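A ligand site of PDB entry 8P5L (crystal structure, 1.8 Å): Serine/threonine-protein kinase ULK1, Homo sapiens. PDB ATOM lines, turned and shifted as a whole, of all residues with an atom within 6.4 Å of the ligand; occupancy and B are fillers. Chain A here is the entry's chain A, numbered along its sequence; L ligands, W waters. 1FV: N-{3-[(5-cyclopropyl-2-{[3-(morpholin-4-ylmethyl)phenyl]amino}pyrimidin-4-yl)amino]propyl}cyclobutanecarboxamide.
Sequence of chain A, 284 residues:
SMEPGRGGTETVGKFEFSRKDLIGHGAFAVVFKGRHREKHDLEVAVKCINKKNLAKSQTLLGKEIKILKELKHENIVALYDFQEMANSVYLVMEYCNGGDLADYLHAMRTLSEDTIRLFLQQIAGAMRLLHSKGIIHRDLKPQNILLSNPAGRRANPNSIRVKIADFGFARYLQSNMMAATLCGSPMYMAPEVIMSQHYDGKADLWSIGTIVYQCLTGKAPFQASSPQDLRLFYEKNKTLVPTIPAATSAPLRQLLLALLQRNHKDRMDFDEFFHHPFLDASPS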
ATOM      1  N   ILE A  23     -30.648 -19.235  -9.044  1.00  0.00           N
ATOM      2  CA  ILE A  23     -30.125 -20.275  -9.907  1.00  0.00           C
ATOM      3  C   ILE A  23     -30.627 -21.623  -9.431  1.00  0.00           C
ATOM      4  O   ILE A  23     -30.295 -22.637 -10.048  1.00  0.00           O
ATOM      5  CB  ILE A  23     -28.599 -20.247 -10.003  1.00  0.00           C
ATOM      6  CG1 ILE A  23     -27.878 -20.269  -8.635  1.00  0.00           C
ATOM      7  CG2 ILE A  23     -28.175 -19.051 -10.826  1.00  0.00           C
ATOM      8  CD1 ILE A  23     -26.394 -20.333  -8.768  1.00  0.00           C
ATOM      9  N   GLY A  24     -31.388 -21.628  -8.327  1.00  0.00           N
ATOM     10  CA  GLY A  24     -32.003 -22.851  -7.861  1.00  0.00           C
ATOM     11  C   GLY A  24     -32.876 -22.624  -6.643  1.00  0.00           C
ATOM     12  O   GLY A  24     -32.708 -21.644  -5.905  1.00  0.00           O
ATOM     13  N   HIS A  25     -33.848 -23.528  -6.458  1.00  0.00           N
ATOM     14  CA  HIS A  25     -34.723 -23.438  -5.310  1.00  0.00           C
ATOM     15  C   HIS A  25     -35.289 -24.826  -4.999  1.00  0.00           C
ATOM     16  O   HIS A  25     -35.447 -25.652  -5.877  1.00  0.00           O
ATOM     17  CB  HIS A  25     -35.815 -22.370  -5.461  1.00  0.00           C
ATOM     18  CG  HIS A  25     -37.018 -22.799  -6.249  1.00  0.00           C
ATOM     19  ND1 HIS A  25     -37.031 -22.849  -7.635  1.00  0.00           N
ATOM     20  CD2 HIS A  25     -38.245 -23.149  -5.838  1.00  0.00           C
ATOM     21  CE1 HIS A  25     -38.225 -23.256  -8.043  1.00  0.00           C
ATOM     22  NE2 HIS A  25     -38.971 -23.444  -6.967  1.00  0.00           N
ATOM     23  N   GLY A  26     -35.524 -25.043  -3.723  1.00  0.00           N
ATOM     24  CA  GLY A  26     -36.268 -26.184  -3.244  1.00  0.00           C
ATOM     25  C   GLY A  26     -37.150 -25.733  -2.097  1.00  0.00           C
ATOM     26  O   GLY A  26     -37.213 -24.549  -1.800  1.00  0.00           O
ATOM     27  N   ALA A  27     -37.805 -26.686  -1.443  1.00  0.00           N
ATOM     28  CA  ALA A  27     -38.722 -26.307  -0.387  1.00  0.00           C
ATOM     29  C   ALA A  27     -37.940 -25.685   0.766  1.00  0.00           C
ATOM     30  O   ALA A  27     -38.515 -24.969   1.588  1.00  0.00           O
ATOM     31  CB  ALA A  27     -39.495 -27.523   0.044  1.00  0.00           C
ATOM     32  N   PHE A  28     -36.637 -25.968   0.877  1.00  0.00           N
ATOM     33  CA  PHE A  28     -35.939 -25.578   2.092  1.00  0.00           C
ATOM     34  C   PHE A  28     -34.710 -24.726   1.827  1.00  0.00           C
ATOM     35  O   PHE A  28     -33.885 -24.552   2.732  1.00  0.00           O
ATOM     36  CB  PHE A  28     -35.537 -26.842   2.862  1.00  0.00           C
ATOM     37  CG  PHE A  28     -36.715 -27.733   3.142  1.00  0.00           C
ATOM     38  CD1 PHE A  28     -37.773 -27.283   3.913  1.00  0.00           C
ATOM     39  CD2 PHE A  28     -36.800 -28.996   2.566  1.00  0.00           C
ATOM     40  CE1 PHE A  28     -38.877 -28.096   4.155  1.00  0.00           C
ATOM     41  CE2 PHE A  28     -37.904 -29.809   2.808  1.00  0.00           C
ATOM     42  CZ  PHE A  28     -38.936 -29.354   3.593  1.00  0.00           C
ATOM     43  N   ALA A  29     -34.580 -24.199   0.602  1.00  0.00           N
ATOM     44  CA  ALA A  29     -33.460 -23.347   0.251  1.00  0.00           C
ATOM     45  C   ALA A  29     -33.692 -22.648  -1.081  1.00  0.00           C
ATOM     46  O   ALA A  29     -34.429 -23.153  -1.942  1.00  0.00           O
ATOM     47  CB  ALA A  29     -32.163 -24.109   0.209  1.00  0.00           C
ATOM     48  N   VAL A  30     -33.040 -21.503  -1.225  1.00  0.00           N
ATOM     49  CA  VAL A  30     -32.931 -20.797  -2.487  1.00  0.00           C
ATOM     50  C   VAL A  30     -31.447 -20.534  -2.696  1.00  0.00           C
ATOM     51  O   VAL A  30     -30.701 -20.395  -1.723  1.00  0.00           O
ATOM     52  CB  VAL A  30     -33.764 -19.487  -2.464  1.00  0.00           C
ATOM     53  CG1 VAL A  30     -35.257 -19.760  -2.340  1.00  0.00           C
ATOM     54  CG2 VAL A  30     -33.302 -18.582  -1.344  1.00  0.00           C
ATOM     55  N   VAL A  31     -31.019 -20.513  -3.955  1.00  0.00           N
ATOM     56  CA  VAL A  31     -29.618 -20.300  -4.257  1.00  0.00           C
ATOM     57  C   VAL A  31     -29.499 -19.137  -5.241  1.00  0.00           C
ATOM     58  O   VAL A  31     -30.183 -19.146  -6.272  1.00  0.00           O
ATOM     59  CB  VAL A  31     -28.963 -21.552  -4.863  1.00  0.00           C
ATOM     60  CG1 VAL A  31     -27.489 -21.340  -5.164  1.00  0.00           C
ATOM     61  CG2 VAL A  31     -29.206 -22.766  -3.952  1.00  0.00           C
ATOM     62  N   LYS A  33     -26.657 -16.584  -7.550  1.00  0.00           N
ATOM     63  CA  LYS A  33     -25.315 -16.354  -8.049  1.00  0.00           C
ATOM     64  C   LYS A  33     -24.744 -15.113  -7.377  1.00  0.00           C
ATOM     65  O   LYS A  33     -25.450 -14.130  -7.174  1.00  0.00           O
ATOM     66  CB  LYS A  33     -25.334 -16.109  -9.553  1.00  0.00           C
ATOM     67  CG  LYS A  33     -24.018 -16.244 -10.291  1.00  0.00           C
ATOM     68  CD  LYS A  33     -24.266 -16.151 -11.776  1.00  0.00           C
ATOM     69  CE  LYS A  33     -23.108 -16.648 -12.582  1.00  0.00           C
ATOM     70  NZ  LYS A  33     -21.926 -15.805 -12.398  1.00  0.00           N
ATOM     71  N   ALA A  45     -22.004 -19.501  -5.469  1.00  0.00           N
ATOM     72  CA  ALA A  45     -23.402 -19.742  -5.248  1.00  0.00           C
ATOM     73  C   ALA A  45     -23.712 -19.523  -3.773  1.00  0.00           C
ATOM     74  O   ALA A  45     -23.100 -20.180  -2.921  1.00  0.00           O
ATOM     75  CB  ALA A  45     -23.706 -21.199  -5.622  1.00  0.00           C
ATOM     76  N   VAL A  46     -24.683 -18.679  -3.489  1.00  0.00           N
ATOM     77  CA  VAL A  46     -25.028 -18.370  -2.111  1.00  0.00           C
ATOM     78  C   VAL A  46     -26.379 -18.980  -1.781  1.00  0.00           C
ATOM     79  O   VAL A  46     -27.429 -18.638  -2.357  1.00  0.00           O
ATOM     80  CB  VAL A  46     -25.019 -16.848  -1.793  1.00  0.00           C
ATOM     81  CG1 VAL A  46     -25.427 -16.608  -0.327  1.00  0.00           C
ATOM     82  CG2 VAL A  46     -23.689 -16.221  -2.087  1.00  0.00           C
ATOM     83  N   LYS A  47     -26.349 -19.944  -0.832  1.00  0.00           N
ATOM     84  CA  LYS A  47     -27.549 -20.635  -0.433  1.00  0.00           C
ATOM     85  C   LYS A  47     -28.147 -19.984   0.809  1.00  0.00           C
ATOM     86  O   LYS A  47     -27.450 -19.811   1.810  1.00  0.00           O
ATOM     87  CB  LYS A  47     -27.185 -22.121  -0.249  1.00  0.00           C
ATOM     88  CG  LYS A  47     -28.334 -23.035   0.083  1.00  0.00           C
ATOM     89  CD  LYS A  47     -27.916 -24.508   0.001  1.00  0.00           C
ATOM     90  CE  LYS A  47     -29.014 -25.473   0.320  1.00  0.00           C
ATOM     91  NZ  LYS A  47     -28.649 -26.850  -0.103  1.00  0.00           N
ATOM     92  N   GLU A  64     -26.157 -28.872   6.832  1.00  0.00           N
ATOM     93  CA  GLU A  64     -25.297 -28.903   5.671  1.00  0.00           C
ATOM     94  C   GLU A  64     -23.937 -28.303   5.973  1.00  0.00           C
ATOM     95  O   GLU A  64     -22.895 -28.809   5.510  1.00  0.00           O
ATOM     96  CB  GLU A  64     -26.022 -28.225   4.489  1.00  0.00           C
ATOM     97  CG  GLU A  64     -25.207 -28.263   3.246  1.00  0.00           C
ATOM     98  CD  GLU A  64     -25.959 -27.960   1.966  1.00  0.00           C
ATOM     99  OE1 GLU A  64     -27.027 -27.303   2.085  1.00  0.00           O
ATOM    100  OE2 GLU A  64     -25.503 -28.449   0.878  1.00  0.00           O
ATOM    101  N   VAL A  77     -19.263 -30.277  -4.148  1.00  0.00           N
ATOM    102  CA  VAL A  77     -19.275 -28.829  -4.234  1.00  0.00           C
ATOM    103  C   VAL A  77     -18.584 -28.251  -2.994  1.00  0.00           C
ATOM    104  O   VAL A  77     -18.863 -28.664  -1.840  1.00  0.00           O
ATOM    105  CB  VAL A  77     -20.722 -28.337  -4.376  1.00  0.00           C
ATOM    106  CG1 VAL A  77     -21.437 -28.349  -3.020  1.00  0.00           C
ATOM    107  CG2 VAL A  77     -20.791 -26.980  -5.017  1.00  0.00           C
ATOM    108  N   ALA A  78     -17.629 -27.366  -3.232  1.00  0.00           N
ATOM    109  CA  ALA A  78     -16.838 -26.778  -2.154  1.00  0.00           C
ATOM    110  C   ALA A  78     -17.651 -25.761  -1.339  1.00  0.00           C
ATOM    111  O   ALA A  78     -18.463 -24.996  -1.858  1.00  0.00           O
ATOM    112  CB  ALA A  78     -15.580 -26.202  -2.735  1.00  0.00           C
ATOM    113  N   MET A  93     -20.884 -21.248  -1.570  1.00  0.00           N
ATOM    114  CA  MET A  93     -20.358 -22.426  -2.222  1.00  0.00           C
ATOM    115  C   MET A  93     -19.827 -22.127  -3.630  1.00  0.00           C
ATOM    116  O   MET A  93     -20.085 -21.081  -4.229  1.00  0.00           O
ATOM    117  CB  MET A  93     -21.490 -23.466  -2.230  1.00  0.00           C
ATOM    118  CG  MET A  93     -21.582 -24.156  -0.768  1.00  0.00           C
ATOM    119  SD  MET A  93     -22.949 -25.159  -0.613  1.00  0.00           S
ATOM    120  CE  MET A  93     -24.329 -24.138  -1.122  1.00  0.00           C
ATOM    121  N   GLU A  94     -18.989 -23.056  -4.079  1.00  0.00           N
ATOM    122  CA  GLU A  94     -18.558 -23.181  -5.452  1.00  0.00           C
ATOM    123  C   GLU A  94     -19.730 -23.019  -6.414  1.00  0.00           C
ATOM    124  O   GLU A  94     -20.794 -23.596  -6.257  1.00  0.00           O
ATOM    125  CB  GLU A  94     -17.842 -24.509  -5.573  1.00  0.00           C
ATOM    126  CG  GLU A  94     -17.469 -24.949  -6.956  1.00  0.00           C
ATOM    127  CD  GLU A  94     -16.738 -26.293  -7.022  1.00  0.00           C
ATOM    128  OE1 GLU A  94     -16.748 -27.122  -6.021  1.00  0.00           O
ATOM    129  OE2 GLU A  94     -16.201 -26.531  -8.068  1.00  0.00           O
ATOM    130  N   TYR A  95     -19.510 -22.169  -7.432  1.00  0.00           N
ATOM    131  CA  TYR A  95     -20.430 -22.027  -8.555  1.00  0.00           C
ATOM    132  C   TYR A  95     -20.000 -22.963  -9.681  1.00  0.00           C
ATOM    133  O   TYR A  95     -18.845 -22.984 -10.096  1.00  0.00           O
ATOM    134  CB  TYR A  95     -20.403 -20.578  -9.058  1.00  0.00           C
ATOM    135  CG  TYR A  95     -21.254 -20.368 -10.291  1.00  0.00           C
ATOM    136  CD1 TYR A  95     -22.625 -20.335 -10.204  1.00  0.00           C
ATOM    137  CD2 TYR A  95     -20.674 -20.156 -11.511  1.00  0.00           C
ATOM    138  CE1 TYR A  95     -23.404 -20.148 -11.325  1.00  0.00           C
ATOM    139  CE2 TYR A  95     -21.442 -20.001 -12.656  1.00  0.00           C
ATOM    140  CZ  TYR A  95     -22.802 -19.932 -12.545  1.00  0.00           C
ATOM    141  OH  TYR A  95     -23.562 -19.752 -13.656  1.00  0.00           O
ATOM    142  N   CYS A  96     -20.930 -23.814 -10.114  1.00  0.00           N
ATOM    143  CA  CYS A  96     -20.703 -24.769 -11.195  1.00  0.00           C
ATOM    144  C   CYS A  96     -21.369 -24.201 -12.472  1.00  0.00           C
ATOM    145  O   CYS A  96     -22.590 -24.163 -12.546  1.00  0.00           O
ATOM    146  CB  CYS A  96     -21.266 -26.137 -10.835  1.00  0.00           C
ATOM    147  SG  CYS A  96     -20.395 -26.781  -9.351  1.00  0.00           S
ATOM    148  N   ASN A  97     -20.552 -23.864 -13.462  1.00  0.00           N
ATOM    149  CA  ASN A  97     -21.027 -23.049 -14.581  1.00  0.00           C
ATOM    150  C   ASN A  97     -21.917 -23.842 -15.557  1.00  0.00           C
ATOM    151  O   ASN A  97     -22.543 -23.231 -16.426  1.00  0.00           O
ATOM    152  CB  ASN A  97     -19.861 -22.398 -15.321  1.00  0.00           C
ATOM    153  CG  ASN A  97     -18.901 -23.394 -15.929  1.00  0.00           C
ATOM    154  OD1 ASN A  97     -19.172 -24.583 -16.034  1.00  0.00           O
ATOM    155  ND2 ASN A  97     -17.737 -22.939 -16.346  1.00  0.00           N
ATOM    156  N   GLY A  98     -21.982 -25.176 -15.423  1.00  0.00           N
ATOM    157  CA  GLY A  98     -22.822 -26.031 -16.272  1.00  0.00           C
ATOM    158  C   GLY A  98     -24.225 -26.336 -15.761  1.00  0.00           C
ATOM    159  O   GLY A  98     -25.019 -26.965 -16.461  1.00  0.00           O
ATOM    160  N   GLY A  99     -24.555 -25.882 -14.568  1.00  0.00           N
ATOM    161  CA  GLY A  99     -25.865 -26.100 -14.019  1.00  0.00           C
ATOM    162  C   GLY A  99     -25.990 -27.588 -13.635  1.00  0.00           C
ATOM    163  O   GLY A  99     -24.987 -28.256 -13.440  1.00  0.00           O
ATOM    164  N   ASP A 100     -27.218 -28.019 -13.420  1.00  0.00           N
ATOM    165  CA  ASP A 100     -27.461 -29.341 -12.867  1.00  0.00           C
ATOM    166  C   ASP A 100     -27.668 -30.413 -13.944  1.00  0.00           C
ATOM    167  O   ASP A 100     -27.933 -30.156 -15.135  1.00  0.00           O
ATOM    168  CB  ASP A 100     -28.589 -29.304 -11.827  1.00  0.00           C
ATOM    169  CG  ASP A 100     -30.048 -29.144 -12.286  1.00  0.00           C
ATOM    170  OD1 ASP A 100     -30.369 -29.480 -13.383  1.00  0.00           O
ATOM    171  OD2 ASP A 100     -30.857 -28.674 -11.485  1.00  0.00           O
ATOM    172  N   ASP A 103     -31.270 -30.508 -15.815  1.00  0.00           N
ATOM    173  CA  ASP A 103     -31.494 -29.655 -16.984  1.00  0.00           C
ATOM    174  C   ASP A 103     -30.674 -30.160 -18.163  1.00  0.00           C
ATOM    175  O   ASP A 103     -31.162 -30.156 -19.274  1.00  0.00           O
ATOM    176  CB  ASP A 103     -31.216 -28.184 -16.706  1.00  0.00           C
ATOM    177  CG  ASP A 103     -32.159 -27.562 -15.702  1.00  0.00           C
ATOM    178  OD1 ASP A 103     -33.281 -28.027 -15.598  1.00  0.00           O
ATOM    179  OD2 ASP A 103     -31.713 -26.655 -14.983  1.00  0.00           O
ATOM    180  N   GLN A 143     -31.146 -33.254 -10.005  1.00  0.00           N
ATOM    181  CA  GLN A 143     -31.252 -31.863  -9.532  1.00  0.00           C
ATOM    182  C   GLN A 143     -30.088 -31.481  -8.607  1.00  0.00           C
ATOM    183  O   GLN A 143     -29.676 -30.323  -8.608  1.00  0.00           O
ATOM    184  CB  GLN A 143     -32.631 -31.601  -8.913  1.00  0.00           C
ATOM    185  CG  GLN A 143     -33.808 -31.760  -9.923  1.00  0.00           C
ATOM    186  CD  GLN A 143     -34.227 -33.179 -10.324  1.00  0.00           C
ATOM    187  OE1 GLN A 143     -33.763 -34.224  -9.873  1.00  0.00           O
ATOM    188  NE2 GLN A 143     -35.146 -33.237 -11.278  1.00  0.00           N
ATOM    189  N   ASN A 144     -29.436 -32.456  -7.955  1.00  0.00           N
ATOM    190  CA  ASN A 144     -28.412 -32.225  -6.955  1.00  0.00           C
ATOM    191  C   ASN A 144     -27.043 -32.637  -7.463  1.00  0.00           C
ATOM    192  O   ASN A 144     -26.093 -32.720  -6.675  1.00  0.00           O
ATOM    193  CB  ASN A 144     -28.714 -32.980  -5.636  1.00  0.00           C
ATOM    194  CG  ASN A 144     -29.802 -32.273  -4.902  1.00  0.00           C
ATOM    195  OD1 ASN A 144     -30.104 -31.095  -5.197  1.00  0.00           O
ATOM    196  ND2 ASN A 144     -30.468 -32.985  -4.016  1.00  0.00           N
ATOM    197  N   ILE A 145     -26.941 -32.960  -8.757  1.00  0.00           N
ATOM    198  CA  ILE A 145     -25.655 -33.246  -9.334  1.00  0.00           C
ATOM    199  C   ILE A 145     -25.289 -32.061 -10.250  1.00  0.00           C
ATOM    200  O   ILE A 145     -26.053 -31.761 -11.187  1.00  0.00           O
ATOM    201  CB  ILE A 145     -25.676 -34.568 -10.125  1.00  0.00           C
ATOM    202  CG1 ILE A 145     -26.112 -35.804  -9.298  1.00  0.00           C
ATOM    203  CG2 ILE A 145     -24.347 -34.790 -10.827  1.00  0.00           C
ATOM    204  CD1 ILE A 145     -25.149 -36.240  -8.288  1.00  0.00           C
ATOM    205  N   LEU A 146     -24.118 -31.448 -10.034  1.00  0.00           N
ATOM    206  CA  LEU A 146     -23.741 -30.255 -10.784  1.00  0.00           C
ATOM    207  C   LEU A 146     -22.642 -30.548 -11.785  1.00  0.00           C
ATOM    208  O   LEU A 146     -21.793 -31.410 -11.562  1.00  0.00           O
ATOM    209  CB  LEU A 146     -23.322 -29.151  -9.814  1.00  0.00           C
ATOM    210  CG  LEU A 146     -24.474 -28.713  -8.905  1.00  0.00           C
ATOM    211  CD1 LEU A 146     -23.964 -27.919  -7.722  1.00  0.00           C
ATOM    212  CD2 LEU A 146     -25.498 -27.922  -9.709  1.00  0.00           C
ATOM    213  N   LEU A 147     -22.631 -29.741 -12.860  1.00  0.00           N
ATOM    214  CA  LEU A 147     -21.620 -29.860 -13.893  1.00  0.00           C
ATOM    215  C   LEU A 147     -20.835 -28.550 -13.992  1.00  0.00           C
ATOM    216  O   LEU A 147     -21.395 -27.469 -13.871  1.00  0.00           O
ATOM    217  CB  LEU A 147     -22.382 -30.144 -15.195  1.00  0.00           C
ATOM    218  CG  LEU A 147     -23.416 -31.274 -15.096  1.00  0.00           C
ATOM    219  CD1 LEU A 147     -24.262 -31.350 -16.351  1.00  0.00           C
ATOM    220  CD2 LEU A 147     -22.717 -32.603 -14.770  1.00  0.00           C
ATOM    221  N   ALA A 165     -23.983 -32.171  -4.777  1.00  0.00           N
ATOM    222  CA  ALA A 165     -24.422 -31.027  -3.986  1.00  0.00           C
ATOM    223  C   ALA A 165     -25.597 -31.371  -3.083  1.00  0.00           C
ATOM    224  O   ALA A 165     -26.092 -32.489  -3.118  1.00  0.00           O
ATOM    225  CB  ALA A 165     -24.824 -29.893  -4.885  1.00  0.00           C
ATOM    226  N   ASP A 166     -25.982 -30.403  -2.214  1.00  0.00           N
ATOM    227  CA  ASP A 166     -27.181 -30.435  -1.380  1.00  0.00           C
ATOM    228  C   ASP A 166     -27.126 -31.545  -0.315  1.00  0.00           C
ATOM    229  O   ASP A 166     -27.811 -32.573  -0.409  1.00  0.00           O
ATOM    230  CB  ASP A 166     -28.443 -30.568  -2.189  1.00  0.00           C
ATOM    231  CG  ASP A 166     -29.639 -30.092  -1.387  1.00  0.00           C
ATOM    232  OD1 ASP A 166     -29.455 -29.782  -0.161  1.00  0.00           O
ATOM    233  OD2 ASP A 166     -30.729 -30.037  -1.979  1.00  0.00           O
HETATM  234  CAM 1FV L   1     -30.554 -26.495  -3.003  1.00  0.00           C
HETATM  235  CAH 1FV L   1     -31.932 -25.838  -3.191  1.00  0.00           C
HETATM  236  CAN 1FV L   1     -31.809 -26.048  -4.708  1.00  0.00           C
HETATM  237  CBF 1FV L   1     -30.638 -27.013  -4.457  1.00  0.00           C
HETATM  238  CAZ 1FV L   1     -29.438 -26.891  -5.353  1.00  0.00           C
HETATM  239  OAA 1FV L   1     -28.345 -26.499  -4.952  1.00  0.00           O
HETATM  240  NAV 1FV L   1     -29.638 -27.254  -6.617  1.00  0.00           N
HETATM  241  CAI 1FV L   1     -28.629 -27.177  -7.670  1.00  0.00           C
HETATM  242  CAG 1FV L   1     -28.769 -25.916  -8.494  1.00  0.00           C
HETATM  243  CAJ 1FV L   1     -28.471 -24.659  -7.662  1.00  0.00           C
HETATM  244  NAW 1FV L   1     -27.174 -24.684  -7.042  1.00  0.00           N
HETATM  245  C4  1FV L   1     -26.003 -24.481  -7.682  1.00  0.00           C
HETATM  246  N3  1FV L   1     -26.028 -24.018  -8.949  1.00  0.00           N
HETATM  247  C5  1FV L   1     -24.814 -24.680  -7.004  1.00  0.00           C
HETATM  248  CBG 1FV L   1     -24.817 -25.291  -5.644  1.00  0.00           C
HETATM  249  CAO 1FV L   1     -23.779 -25.066  -4.610  1.00  0.00           C
HETATM  250  CAP 1FV L   1     -25.169 -24.598  -4.378  1.00  0.00           C
HETATM  251  C6  1FV L   1     -23.636 -24.427  -7.684  1.00  0.00           C
HETATM  252  N1  1FV L   1     -23.625 -23.992  -8.960  1.00  0.00           N
HETATM  253  C2  1FV L   1     -24.835 -23.826  -9.536  1.00  0.00           C
HETATM  254  NAX 1FV L   1     -24.817 -23.426 -10.821  1.00  0.00           N
HETATM  255  CBB 1FV L   1     -25.837 -23.143 -11.764  1.00  0.00           C
HETATM  256  CAF 1FV L   1     -25.424 -22.554 -12.963  1.00  0.00           C
HETATM  257  CAD 1FV L   1     -27.183 -23.443 -11.564  1.00  0.00           C
HETATM  258  CAB 1FV L   1     -28.105 -23.141 -12.544  1.00  0.00           C
HETATM  259  CAC 1FV L   1     -27.682 -22.511 -13.710  1.00  0.00           C
HETATM  260  CBA 1FV L   1     -26.347 -22.266 -13.971  1.00  0.00           C
HETATM  261  CAS 1FV L   1     -25.920 -21.488 -15.195  1.00  0.00           C
HETATM  262  NBH 1FV L   1     -25.777 -22.118 -16.512  1.00  0.00           N
HETATM  263  CAQ 1FV L   1     -26.544 -23.317 -16.768  1.00  0.00           C
HETATM  264  CAK 1FV L   1     -26.028 -23.961 -18.031  1.00  0.00           C
HETATM  265  OAY 1FV L   1     -26.078 -23.099 -19.163  1.00  0.00           O
HETATM  266  CAL 1FV L   1     -25.647 -21.742 -18.919  1.00  0.00           C
HETATM  267  CAR 1FV L   1     -26.053 -21.168 -17.589  1.00  0.00           C
HETATM  268  O   HOH W   1     -28.909 -21.049 -16.781  1.00  0.00           O
HETATM  269  O   HOH W   2     -28.740 -25.449 -16.080  1.00  0.00           O
HETATM  270  O   HOH W   3     -29.497 -26.110 -13.366  1.00  0.00           O
HETATM  271  O   HOH W   4     -31.819 -27.604  -0.031  1.00  0.00           O
HETATM  272  O   HOH W   5     -27.270 -27.153  -2.511  1.00  0.00           O
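Water W5 lies within hydrogen-bond range of an oxygen (OAA) of the ligand (2.7 Å) and the side-chain amino group (NZ) of Lys 47 (2.8 Å).
Water W3 lies within hydrogen-bond range of the side-chain carboxylate of Asp 103 (2.8 Å) and the backbone NH of Asp 100 (3.0 Å).
Water W4 bridges OD1 of Asp 166 (3.2 Å) and NZ of Lys 47 (3.3 Å).
The backbone carbonyl oxygen (O) of Val 31 is in hydrogen-bond range of the backbone NH (N) of Ile 23 (2.8 Å).
The backbone carbonyl oxygen (O) of Leu 147 sits at hydrogen-bond distance from the backbone NH (N) of Gly 98 (2.8 Å).
OD2 of Asp 166 lies close to OD1 of Asn 144 (3.4 Å).
OE1 of Glu 64 lies within salt-bridge range of NZ of Lys 47 (2.8 Å).
The backbone NH of Val 31 lies within hydrogen-bond range of the backbone carbonyl oxygen of Gly 24.
The side-chain amino group (NZ) of Lys 47 lies within salt-bridge range of the side-chain carboxylate (OD1) of Asp 166.
O of Gly 99 sits at hydrogen-bond distance from N of Leu 147.
The backbone NH of Ala 78 is in hydrogen-bond range of the side-chain carboxylate of Glu 94.
Ile 23 touches the ligand.
Gly 24 touches the ligand (CA to CAJ, 3.97 Å).
His 25 touches the ligand (N to CAN, 3.7 Å).
Gly 26 touches the ligand.
Ala 29 touches the ligand.
CG1 of Val 31 touches NAW of the ligand, 3.8 Å away.
Ala 45 touches the ligand (CB to C6, 3.8 Å).
Lys 47 touches the ligand (NZ to CAM, 3.5 Å).
CG2 of Val 77 touches CAO of the ligand, at 3.6 Å.
Met 93 touches the ligand (CE to CAP, 3.4 Å).
Glu 94 touches the ligand.
Tyr 95 touches the ligand.
Gly 98 touches the ligand (O to CAK, 3.5 Å).
Gly 99 touches the ligand.
O of Gln 143 touches CAI of the ligand, 3.4 Å away.
Leu 146 touches the ligand (CD1 to C5, 3.4 Å).
Asp 166 touches the ligand.
Hydrophobic or aromatic side chains that line the ligand: Ile 23, Ala 29, Val 31, Ala 45, Val 77, Met 93, Tyr 95 and Leu 146.
Within 4 Å of the ligand: Ile 23, Gly 24, His 25, Gly 26, Ala 29, Val 31, Ala 45, Lys 47, Val 77, Met 93, Glu 94, Tyr 95, Cys 96, Asn 97, Gly 98, Gly 99, Gln 143, Leu 146 and Asp 166.
The nearest printed residue that does not touch the ligand is Asn 144 (4.1 Å).
O of Asn 97 lies close to NBH of the ligand (3.4 Å).
O of Cys 96 is in hydrogen-bond range of NAX of the ligand, at 2.9 Å.
The backbone NH (N) of Cys 96 lies within hydrogen-bond range of a nitrogen (N1) of the ligand (2.9 Å).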
